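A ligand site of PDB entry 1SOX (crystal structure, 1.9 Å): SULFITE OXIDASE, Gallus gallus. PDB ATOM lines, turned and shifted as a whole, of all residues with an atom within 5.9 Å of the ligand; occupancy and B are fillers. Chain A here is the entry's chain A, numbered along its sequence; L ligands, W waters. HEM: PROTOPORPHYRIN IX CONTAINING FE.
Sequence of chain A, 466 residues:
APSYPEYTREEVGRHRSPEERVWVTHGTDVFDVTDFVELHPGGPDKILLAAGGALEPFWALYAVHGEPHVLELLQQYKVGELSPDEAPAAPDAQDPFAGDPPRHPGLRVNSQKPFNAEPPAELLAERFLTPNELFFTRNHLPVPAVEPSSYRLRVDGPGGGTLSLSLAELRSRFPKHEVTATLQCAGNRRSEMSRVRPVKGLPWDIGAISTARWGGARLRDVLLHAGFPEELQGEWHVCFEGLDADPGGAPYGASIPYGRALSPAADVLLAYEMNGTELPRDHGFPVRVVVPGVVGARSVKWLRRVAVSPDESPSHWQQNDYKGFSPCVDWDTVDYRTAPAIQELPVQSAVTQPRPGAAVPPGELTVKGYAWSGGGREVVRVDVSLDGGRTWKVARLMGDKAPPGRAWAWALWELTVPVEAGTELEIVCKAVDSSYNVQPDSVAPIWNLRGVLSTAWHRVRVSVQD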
ATOM      1  N   VAL A  24      15.397 -16.317   1.481  1.00  0.00           N
ATOM      2  CA  VAL A  24      14.689 -15.846   2.674  1.00  0.00           C
ATOM      3  C   VAL A  24      13.597 -16.853   3.016  1.00  0.00           C
ATOM      4  O   VAL A  24      13.245 -17.709   2.201  1.00  0.00           O
ATOM      5  CB  VAL A  24      14.089 -14.443   2.523  1.00  0.00           C
ATOM      6  CG1 VAL A  24      15.132 -13.360   2.346  1.00  0.00           C
ATOM      7  CG2 VAL A  24      13.112 -14.449   1.339  1.00  0.00           C
ATOM      8  N   VAL A  33      15.030 -15.110  -3.773  1.00  0.00           N
ATOM      9  CA  VAL A  33      14.587 -13.835  -4.305  1.00  0.00           C
ATOM     10  C   VAL A  33      15.686 -13.025  -4.961  1.00  0.00           C
ATOM     11  O   VAL A  33      15.573 -11.807  -5.156  1.00  0.00           O
ATOM     12  CB  VAL A  33      13.924 -12.987  -3.191  1.00  0.00           C
ATOM     13  CG1 VAL A  33      12.743 -13.751  -2.581  1.00  0.00           C
ATOM     14  CG2 VAL A  33      14.923 -12.624  -2.112  1.00  0.00           C
ATOM     15  N   PHE A  36      14.434 -10.996  -7.715  1.00  0.00           N
ATOM     16  CA  PHE A  36      13.422 -10.046  -7.294  1.00  0.00           C
ATOM     17  C   PHE A  36      13.978  -8.762  -6.692  1.00  0.00           C
ATOM     18  O   PHE A  36      13.365  -7.704  -6.807  1.00  0.00           O
ATOM     19  CB  PHE A  36      12.472 -10.684  -6.269  1.00  0.00           C
ATOM     20  CG  PHE A  36      11.424  -9.713  -5.814  1.00  0.00           C
ATOM     21  CD1 PHE A  36      10.380  -9.343  -6.646  1.00  0.00           C
ATOM     22  CD2 PHE A  36      11.494  -9.149  -4.551  1.00  0.00           C
ATOM     23  CE1 PHE A  36       9.422  -8.437  -6.213  1.00  0.00           C
ATOM     24  CE2 PHE A  36      10.549  -8.247  -4.123  1.00  0.00           C
ATOM     25  CZ  PHE A  36       9.506  -7.887  -4.945  1.00  0.00           C
ATOM     26  N   HIS A  40      12.067  -4.884  -6.387  1.00  0.00           N
ATOM     27  CA  HIS A  40      11.486  -4.423  -5.138  1.00  0.00           C
ATOM     28  C   HIS A  40      11.277  -2.925  -5.069  1.00  0.00           C
ATOM     29  O   HIS A  40      12.222  -2.135  -5.160  1.00  0.00           O
ATOM     30  CB  HIS A  40      12.416  -4.817  -3.965  1.00  0.00           C
ATOM     31  CG  HIS A  40      11.766  -4.576  -2.634  1.00  0.00           C
ATOM     32  ND1 HIS A  40      12.200  -3.622  -1.755  1.00  0.00           N
ATOM     33  CD2 HIS A  40      10.711  -5.188  -2.051  1.00  0.00           C
ATOM     34  CE1 HIS A  40      11.424  -3.649  -0.681  1.00  0.00           C
ATOM     35  NE2 HIS A  40      10.508  -4.597  -0.830  1.00  0.00           N
ATOM     36  N   PRO A  41      10.055  -2.522  -4.778  1.00  0.00           N
ATOM     37  CA  PRO A  41       9.689  -1.132  -4.609  1.00  0.00           C
ATOM     38  C   PRO A  41      10.589  -0.483  -3.571  1.00  0.00           C
ATOM     39  O   PRO A  41      10.850  -1.090  -2.524  1.00  0.00           O
ATOM     40  CB  PRO A  41       8.206  -1.113  -4.183  1.00  0.00           C
ATOM     41  CG  PRO A  41       7.734  -2.452  -4.729  1.00  0.00           C
ATOM     42  CD  PRO A  41       8.899  -3.411  -4.611  1.00  0.00           C
ATOM     43  N   GLY A  42      11.100   0.707  -3.852  1.00  0.00           N
ATOM     44  CA  GLY A  42      11.959   1.429  -2.936  1.00  0.00           C
ATOM     45  C   GLY A  42      13.422   1.027  -2.960  1.00  0.00           C
ATOM     46  O   GLY A  42      14.216   1.506  -2.139  1.00  0.00           O
ATOM     47  N   GLY A  43      13.823   0.152  -3.877  1.00  0.00           N
ATOM     48  CA  GLY A  43      15.209  -0.277  -3.985  1.00  0.00           C
ATOM     49  C   GLY A  43      15.521  -1.543  -3.205  1.00  0.00           C
ATOM     50  O   GLY A  43      14.694  -2.126  -2.513  1.00  0.00           O
ATOM     51  N   LYS A  46      16.613  -2.121   1.761  1.00  0.00           N
ATOM     52  CA  LYS A  46      15.876  -2.731   2.856  1.00  0.00           C
ATOM     53  C   LYS A  46      15.652  -4.213   2.685  1.00  0.00           C
ATOM     54  O   LYS A  46      15.939  -4.998   3.600  1.00  0.00           O
ATOM     55  CB  LYS A  46      14.511  -2.031   3.023  1.00  0.00           C
ATOM     56  CG  LYS A  46      14.685  -0.517   3.143  1.00  0.00           C
ATOM     57  CD  LYS A  46      15.147  -0.140   4.529  1.00  0.00           C
ATOM     58  CE  LYS A  46      14.252   0.932   5.130  1.00  0.00           C
ATOM     59  NZ  LYS A  46      14.939   2.259   5.173  1.00  0.00           N
ATOM     60  N   ILE A  47      15.172  -4.640   1.518  1.00  0.00           N
ATOM     61  CA  ILE A  47      14.931  -6.070   1.300  1.00  0.00           C
ATOM     62  C   ILE A  47      16.156  -6.922   1.521  1.00  0.00           C
ATOM     63  O   ILE A  47      16.083  -8.012   2.101  1.00  0.00           O
ATOM     64  CB  ILE A  47      14.348  -6.337  -0.095  1.00  0.00           C
ATOM     65  CG1 ILE A  47      14.178  -7.846  -0.289  1.00  0.00           C
ATOM     66  CG2 ILE A  47      15.202  -5.724  -1.191  1.00  0.00           C
ATOM     67  CD1 ILE A  47      13.122  -8.203  -1.318  1.00  0.00           C
ATOM     68  N   LEU A  48      17.357  -6.444   1.156  1.00  0.00           N
ATOM     69  CA  LEU A  48      18.581  -7.217   1.355  1.00  0.00           C
ATOM     70  C   LEU A  48      18.931  -7.393   2.817  1.00  0.00           C
ATOM     71  O   LEU A  48      19.725  -8.260   3.189  1.00  0.00           O
ATOM     72  CB  LEU A  48      19.771  -6.614   0.622  1.00  0.00           C
ATOM     73  CG  LEU A  48      19.801  -6.774  -0.906  1.00  0.00           C
ATOM     74  CD1 LEU A  48      20.908  -5.903  -1.503  1.00  0.00           C
ATOM     75  CD2 LEU A  48      19.989  -8.230  -1.293  1.00  0.00           C
ATOM     76  N   LEU A  49      18.303  -6.653   3.729  1.00  0.00           N
ATOM     77  CA  LEU A  49      18.518  -6.819   5.156  1.00  0.00           C
ATOM     78  C   LEU A  49      18.015  -8.155   5.649  1.00  0.00           C
ATOM     79  O   LEU A  49      18.448  -8.643   6.691  1.00  0.00           O
ATOM     80  CB  LEU A  49      17.823  -5.709   5.927  1.00  0.00           C
ATOM     81  CG  LEU A  49      18.595  -4.507   6.437  1.00  0.00           C
ATOM     82  CD1 LEU A  49      19.814  -4.142   5.604  1.00  0.00           C
ATOM     83  CD2 LEU A  49      17.656  -3.305   6.552  1.00  0.00           C
ATOM     84  N   ALA A  50      17.104  -8.803   4.935  1.00  0.00           N
ATOM     85  CA  ALA A  50      16.565 -10.094   5.300  1.00  0.00           C
ATOM     86  C   ALA A  50      17.391 -11.266   4.778  1.00  0.00           C
ATOM     87  O   ALA A  50      17.041 -12.413   5.081  1.00  0.00           O
ATOM     88  CB  ALA A  50      15.139 -10.195   4.739  1.00  0.00           C
ATOM     89  N   LEU A  55      11.448 -13.549   6.969  1.00  0.00           N
ATOM     90  CA  LEU A  55      10.811 -12.272   6.604  1.00  0.00           C
ATOM     91  C   LEU A  55       9.925 -11.737   7.713  1.00  0.00           C
ATOM     92  O   LEU A  55       9.641 -10.540   7.828  1.00  0.00           O
ATOM     93  CB  LEU A  55      10.004 -12.517   5.323  1.00  0.00           C
ATOM     94  CG  LEU A  55      10.831 -12.714   4.053  1.00  0.00           C
ATOM     95  CD1 LEU A  55       9.970 -13.151   2.879  1.00  0.00           C
ATOM     96  CD2 LEU A  55      11.590 -11.441   3.706  1.00  0.00           C
ATOM     97  N   PHE A  58      10.406  -8.291   9.471  1.00  0.00           N
ATOM     98  CA  PHE A  58      10.231  -7.188   8.531  1.00  0.00           C
ATOM     99  C   PHE A  58       8.770  -7.047   8.134  1.00  0.00           C
ATOM    100  O   PHE A  58       8.294  -5.906   7.945  1.00  0.00           O
ATOM    101  CB  PHE A  58      11.122  -7.334   7.291  1.00  0.00           C
ATOM    102  CG  PHE A  58      12.529  -7.716   7.683  1.00  0.00           C
ATOM    103  CD1 PHE A  58      13.378  -6.785   8.250  1.00  0.00           C
ATOM    104  CD2 PHE A  58      12.964  -9.012   7.525  1.00  0.00           C
ATOM    105  CE1 PHE A  58      14.651  -7.142   8.641  1.00  0.00           C
ATOM    106  CE2 PHE A  58      14.244  -9.375   7.919  1.00  0.00           C
ATOM    107  CZ  PHE A  58      15.106  -8.449   8.481  1.00  0.00           C
ATOM    108  N   TRP A  59       8.031  -8.145   8.049  1.00  0.00           N
ATOM    109  CA  TRP A  59       6.604  -8.106   7.796  1.00  0.00           C
ATOM    110  C   TRP A  59       5.876  -7.400   8.950  1.00  0.00           C
ATOM    111  O   TRP A  59       4.789  -6.830   8.788  1.00  0.00           O
ATOM    112  CB  TRP A  59       5.987  -9.492   7.689  1.00  0.00           C
ATOM    113  CG  TRP A  59       5.812 -10.094   6.343  1.00  0.00           C
ATOM    114  CD1 TRP A  59       4.803 -10.943   5.977  1.00  0.00           C
ATOM    115  CD2 TRP A  59       6.654  -9.953   5.194  1.00  0.00           C
ATOM    116  NE1 TRP A  59       4.961 -11.319   4.660  1.00  0.00           N
ATOM    117  CE2 TRP A  59       6.090 -10.728   4.166  1.00  0.00           C
ATOM    118  CE3 TRP A  59       7.821  -9.221   4.946  1.00  0.00           C
ATOM    119  CZ2 TRP A  59       6.654 -10.813   2.884  1.00  0.00           C
ATOM    120  CZ3 TRP A  59       8.383  -9.298   3.690  1.00  0.00           C
ATOM    121  CH2 TRP A  59       7.804 -10.096   2.682  1.00  0.00           C
ATOM    122  N   LEU A  61       7.235  -4.930  10.677  1.00  0.00           N
ATOM    123  CA  LEU A  61       7.506  -3.516  10.526  1.00  0.00           C
ATOM    124  C   LEU A  61       6.644  -2.896   9.431  1.00  0.00           C
ATOM    125  O   LEU A  61       6.176  -1.770   9.588  1.00  0.00           O
ATOM    126  CB  LEU A  61       8.983  -3.256  10.168  1.00  0.00           C
ATOM    127  CG  LEU A  61       9.985  -3.707  11.240  1.00  0.00           C
ATOM    128  CD1 LEU A  61      11.392  -3.429  10.743  1.00  0.00           C
ATOM    129  CD2 LEU A  61       9.705  -3.033  12.569  1.00  0.00           C
ATOM    130  N   TYR A  62       6.506  -3.591   8.315  1.00  0.00           N
ATOM    131  CA  TYR A  62       5.756  -3.125   7.151  1.00  0.00           C
ATOM    132  C   TYR A  62       4.652  -4.105   6.819  1.00  0.00           C
ATOM    133  O   TYR A  62       4.786  -4.992   5.968  1.00  0.00           O
ATOM    134  CB  TYR A  62       6.726  -2.936   5.975  1.00  0.00           C
ATOM    135  CG  TYR A  62       7.924  -2.074   6.293  1.00  0.00           C
ATOM    136  CD1 TYR A  62       7.807  -0.701   6.410  1.00  0.00           C
ATOM    137  CD2 TYR A  62       9.175  -2.636   6.532  1.00  0.00           C
ATOM    138  CE1 TYR A  62       8.894   0.098   6.710  1.00  0.00           C
ATOM    139  CE2 TYR A  62      10.264  -1.846   6.843  1.00  0.00           C
ATOM    140  CZ  TYR A  62      10.133  -0.485   6.931  1.00  0.00           C
ATOM    141  OH  TYR A  62      11.207   0.318   7.236  1.00  0.00           O
ATOM    142  N   VAL A  64       2.056  -4.146   5.031  1.00  0.00           N
ATOM    143  CA  VAL A  64       1.513  -4.265   3.673  1.00  0.00           C
ATOM    144  C   VAL A  64       1.931  -5.578   3.044  1.00  0.00           C
ATOM    145  O   VAL A  64       1.246  -6.198   2.225  1.00  0.00           O
ATOM    146  CB  VAL A  64       1.952  -3.075   2.807  1.00  0.00           C
ATOM    147  CG1 VAL A  64       3.451  -3.115   2.544  1.00  0.00           C
ATOM    148  CG2 VAL A  64       1.173  -3.111   1.485  1.00  0.00           C
ATOM    149  N   HIS A  65       3.076  -6.136   3.454  1.00  0.00           N
ATOM    150  CA  HIS A  65       3.571  -7.399   2.932  1.00  0.00           C
ATOM    151  C   HIS A  65       2.705  -8.586   3.323  1.00  0.00           C
ATOM    152  O   HIS A  65       2.827  -9.649   2.698  1.00  0.00           O
ATOM    153  CB  HIS A  65       4.994  -7.674   3.392  1.00  0.00           C
ATOM    154  CG  HIS A  65       5.992  -6.660   2.940  1.00  0.00           C
ATOM    155  ND1 HIS A  65       6.338  -5.567   3.688  1.00  0.00           N
ATOM    156  CD2 HIS A  65       6.763  -6.615   1.816  1.00  0.00           C
ATOM    157  CE1 HIS A  65       7.259  -4.879   3.045  1.00  0.00           C
ATOM    158  NE2 HIS A  65       7.555  -5.491   1.900  1.00  0.00           N
ATOM    159  N   GLU A  67      -0.531  -8.583   2.982  1.00  0.00           N
ATOM    160  CA  GLU A  67      -1.696  -8.598   2.074  1.00  0.00           C
ATOM    161  C   GLU A  67      -1.553  -9.624   0.975  1.00  0.00           C
ATOM    162  O   GLU A  67      -0.434  -9.994   0.551  1.00  0.00           O
ATOM    163  CB  GLU A  67      -1.802  -7.168   1.531  1.00  0.00           C
ATOM    164  CG  GLU A  67      -2.385  -6.221   2.576  1.00  0.00           C
ATOM    165  CD  GLU A  67      -2.360  -4.775   2.141  1.00  0.00           C
ATOM    166  OE1 GLU A  67      -2.597  -4.491   0.944  1.00  0.00           O
ATOM    167  OE2 GLU A  67      -2.097  -3.903   3.001  1.00  0.00           O
ATOM    168  N   HIS A  69      -1.853  -9.699  -2.326  1.00  0.00           N
ATOM    169  CA  HIS A  69      -1.075  -9.419  -3.522  1.00  0.00           C
ATOM    170  C   HIS A  69       0.417  -9.546  -3.280  1.00  0.00           C
ATOM    171  O   HIS A  69       1.151  -9.907  -4.198  1.00  0.00           O
ATOM    172  CB  HIS A  69      -1.412  -8.056  -4.111  1.00  0.00           C
ATOM    173  CG  HIS A  69      -0.928  -6.866  -3.337  1.00  0.00           C
ATOM    174  ND1 HIS A  69      -1.418  -6.500  -2.110  1.00  0.00           N
ATOM    175  CD2 HIS A  69       0.022  -5.954  -3.655  1.00  0.00           C
ATOM    176  CE1 HIS A  69      -0.814  -5.406  -1.693  1.00  0.00           C
ATOM    177  NE2 HIS A  69       0.066  -5.054  -2.608  1.00  0.00           N
ATOM    178  N   VAL A  70       0.907  -9.185  -2.079  1.00  0.00           N
ATOM    179  CA  VAL A  70       2.352  -9.305  -1.845  1.00  0.00           C
ATOM    180  C   VAL A  70       2.706 -10.769  -1.655  1.00  0.00           C
ATOM    181  O   VAL A  70       3.687 -11.262  -2.208  1.00  0.00           O
ATOM    182  CB  VAL A  70       2.836  -8.484  -0.648  1.00  0.00           C
ATOM    183  CG1 VAL A  70       4.332  -8.694  -0.398  1.00  0.00           C
ATOM    184  CG2 VAL A  70       2.576  -7.002  -0.891  1.00  0.00           C
ATOM    185  N   LEU A  73       2.889 -12.556  -4.886  1.00  0.00           N
ATOM    186  CA  LEU A  73       4.137 -12.239  -5.584  1.00  0.00           C
ATOM    187  C   LEU A  73       5.303 -13.050  -5.034  1.00  0.00           C
ATOM    188  O   LEU A  73       6.061 -13.662  -5.782  1.00  0.00           O
ATOM    189  CB  LEU A  73       4.392 -10.740  -5.487  1.00  0.00           C
ATOM    190  CG  LEU A  73       5.756 -10.220  -5.947  1.00  0.00           C
ATOM    191  CD1 LEU A  73       5.931 -10.379  -7.442  1.00  0.00           C
ATOM    192  CD2 LEU A  73       5.907  -8.750  -5.544  1.00  0.00           C
ATOM    193  N   LEU A  74       5.410 -13.132  -3.711  1.00  0.00           N
ATOM    194  CA  LEU A  74       6.426 -13.900  -3.006  1.00  0.00           C
ATOM    195  C   LEU A  74       6.416 -15.367  -3.393  1.00  0.00           C
ATOM    196  O   LEU A  74       7.483 -15.910  -3.700  1.00  0.00           O
ATOM    197  CB  LEU A  74       6.236 -13.793  -1.491  1.00  0.00           C
ATOM    198  CG  LEU A  74       7.181 -14.566  -0.580  1.00  0.00           C
ATOM    199  CD1 LEU A  74       8.626 -14.143  -0.750  1.00  0.00           C
ATOM    200  CD2 LEU A  74       6.759 -14.396   0.874  1.00  0.00           C
ATOM    201  N   TYR A  77       8.683 -16.960  -6.126  1.00  0.00           N
ATOM    202  CA  TYR A  77      10.074 -17.251  -5.843  1.00  0.00           C
ATOM    203  C   TYR A  77      10.345 -18.422  -4.910  1.00  0.00           C
ATOM    204  O   TYR A  77      11.497 -18.569  -4.475  1.00  0.00           O
ATOM    205  CB  TYR A  77      10.699 -15.952  -5.274  1.00  0.00           C
ATOM    206  CG  TYR A  77      10.619 -14.850  -6.313  1.00  0.00           C
ATOM    207  CD1 TYR A  77      11.534 -14.786  -7.358  1.00  0.00           C
ATOM    208  CD2 TYR A  77       9.601 -13.913  -6.274  1.00  0.00           C
ATOM    209  CE1 TYR A  77      11.450 -13.788  -8.308  1.00  0.00           C
ATOM    210  CE2 TYR A  77       9.505 -12.911  -7.219  1.00  0.00           C
ATOM    211  CZ  TYR A  77      10.426 -12.860  -8.237  1.00  0.00           C
ATOM    212  OH  TYR A  77      10.338 -11.868  -9.194  1.00  0.00           O
ATOM    213  N   LEU A 123      16.010   0.494  10.641  1.00  0.00           N
ATOM    214  CA  LEU A 123      14.790  -0.139  11.047  1.00  0.00           C
ATOM    215  C   LEU A 123      14.332   0.163  12.474  1.00  0.00           C
ATOM    216  O   LEU A 123      13.149  -0.071  12.764  1.00  0.00           O
ATOM    217  CB  LEU A 123      14.931  -1.653  10.892  1.00  0.00           C
ATOM    218  CG  LEU A 123      15.251  -2.148   9.496  1.00  0.00           C
ATOM    219  CD1 LEU A 123      15.336  -3.679   9.516  1.00  0.00           C
ATOM    220  CD2 LEU A 123      14.223  -1.695   8.457  1.00  0.00           C
HETATM  221  CHA HEM L   1       7.098  -2.343  -0.347  1.00  0.00           C
HETATM  222  CHB HEM L   1       7.481  -6.890  -1.932  1.00  0.00           C
HETATM  223  CHC HEM L   1      10.820  -7.781   1.409  1.00  0.00           C
HETATM  224  CHD HEM L   1      10.594  -3.174   2.849  1.00  0.00           C
HETATM  225  C1A HEM L   1       6.857  -3.516  -1.044  1.00  0.00           C
HETATM  226  C2A HEM L   1       5.824  -3.728  -2.036  1.00  0.00           C
HETATM  227  C3A HEM L   1       5.923  -4.982  -2.477  1.00  0.00           C
HETATM  228  C4A HEM L   1       7.036  -5.603  -1.772  1.00  0.00           C
HETATM  229  CMA HEM L   1       5.063  -5.705  -3.540  1.00  0.00           C
HETATM  230  CAA HEM L   1       4.787  -2.636  -2.413  1.00  0.00           C
HETATM  231  CBA HEM L   1       3.518  -2.753  -1.545  1.00  0.00           C
HETATM  232  CGA HEM L   1       2.337  -1.881  -1.870  1.00  0.00           C
HETATM  233  O1A HEM L   1       2.294  -0.742  -1.338  1.00  0.00           O
HETATM  234  O2A HEM L   1       1.452  -2.341  -2.634  1.00  0.00           O
HETATM  235  C1B HEM L   1       8.414  -7.551  -1.157  1.00  0.00           C
HETATM  236  C2B HEM L   1       8.758  -8.948  -1.253  1.00  0.00           C
HETATM  237  C3B HEM L   1       9.690  -9.190  -0.337  1.00  0.00           C
HETATM  238  C4B HEM L   1       9.942  -7.957   0.367  1.00  0.00           C
HETATM  239  CMB HEM L   1       8.122  -9.932  -2.274  1.00  0.00           C
HETATM  240  CAB HEM L   1      10.416 -10.522  -0.005  1.00  0.00           C
HETATM  241  CBB HEM L   1      10.994 -11.205  -1.014  1.00  0.00           C
HETATM  242  C1C HEM L   1      11.019  -6.624   2.136  1.00  0.00           C
HETATM  243  C2C HEM L   1      11.873  -6.493   3.314  1.00  0.00           C
HETATM  244  C3C HEM L   1      11.809  -5.222   3.709  1.00  0.00           C
HETATM  245  C4C HEM L   1      10.920  -4.526   2.797  1.00  0.00           C
HETATM  246  CMC HEM L   1      12.650  -7.669   3.934  1.00  0.00           C
HETATM  247  CAC HEM L   1      12.481  -4.519   4.911  1.00  0.00           C
HETATM  248  CBC HEM L   1      13.553  -5.013   5.515  1.00  0.00           C
HETATM  249  C1D HEM L   1       9.648  -2.509   2.078  1.00  0.00           C
HETATM  250  C2D HEM L   1       9.344  -1.097   2.146  1.00  0.00           C
HETATM  251  C3D HEM L   1       8.368  -0.847   1.252  1.00  0.00           C
HETATM  252  C4D HEM L   1       8.048  -2.120   0.625  1.00  0.00           C
HETATM  253  CMD HEM L   1      10.078  -0.139   3.112  1.00  0.00           C
HETATM  254  CAD HEM L   1       7.670   0.483   0.954  1.00  0.00           C
HETATM  255  CBD HEM L   1       7.598   1.287  -0.318  1.00  0.00           C
HETATM  256  CGD HEM L   1       8.829   2.011  -0.785  1.00  0.00           C
HETATM  257  O1D HEM L   1       8.780   3.233  -1.062  1.00  0.00           O
HETATM  258  O2D HEM L   1       9.854   1.267  -0.848  1.00  0.00           O
HETATM  259  NA  HEM L   1       7.596  -4.687  -0.904  1.00  0.00           N
HETATM  260  NB  HEM L   1       9.146  -6.938  -0.145  1.00  0.00           N
HETATM  261  NC  HEM L   1      10.451  -5.395   1.845  1.00  0.00           N
HETATM  262  ND  HEM L   1       8.850  -3.136   1.129  1.00  0.00           N
HETATM  263 FE   HEM L   1       9.005  -5.044   0.495  1.00  0.00          FE
HETATM  264  O   HOH W   1      12.078  -0.598   0.004  1.00  0.00           O
HETATM  265  O   HOH W   2       4.447   0.132   0.308  1.00  0.00           O
HETATM  266  O   HOH W   3      12.228   2.256   1.096  1.00  0.00           O
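Residues that only touch the ligand: Lys 46 (3.1 Å), Phe 58 (3.3 Å), Phe 36 (3.5 Å), Val 33 (3.5 Å), Ile 47 (3.6 Å), Ala 50 (3.6 Å), Trp 59 (3.7 Å), Leu 73 (3.7 Å), Val 64 (3.8 Å), Leu 74 (3.8 Å), Tyr 62 (3.8 Å), Val 70 (3.9 Å) and Leu 55 (3.9 Å). Of the 26 residues printed, 18 come within 4 Å of the ligand.
Water W1 lies within hydrogen-bond range of the backbone carbonyl oxygen (O) of Pro 41 (2.9 Å), an oxygen (O2D) of the ligand (3.0 Å) and a ring nitrogen (ND1) of His 40 (3.5 Å).
FE of the ligand is bound by NE2 of His 40 (2.1 Å). FE of the ligand is bound by NE2 of His 65 (2.1 Å). The backbone NH of Gly 42 lies close to an oxygen (O2D) of the ligand (3.3 Å). A ring nitrogen (NE2) of His 69 lies within hydrogen-bond range of an oxygen (O2A) of the ligand, at 3.0 Å. An oxygen (O2D) of the ligand lies close to the backbone carbonyl oxygen (O) of Pro 41 (3.1 Å).
ND1 of His 40 lies within hydrogen-bond range of O of Gly 43, 3.0 Å away. O of His 65 sits at hydrogen-bond distance from NE1 of Trp 59 (3.3 Å). ND1 of His 65 sits at hydrogen-bond distance from O of Tyr 62, 2.8 Å away.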
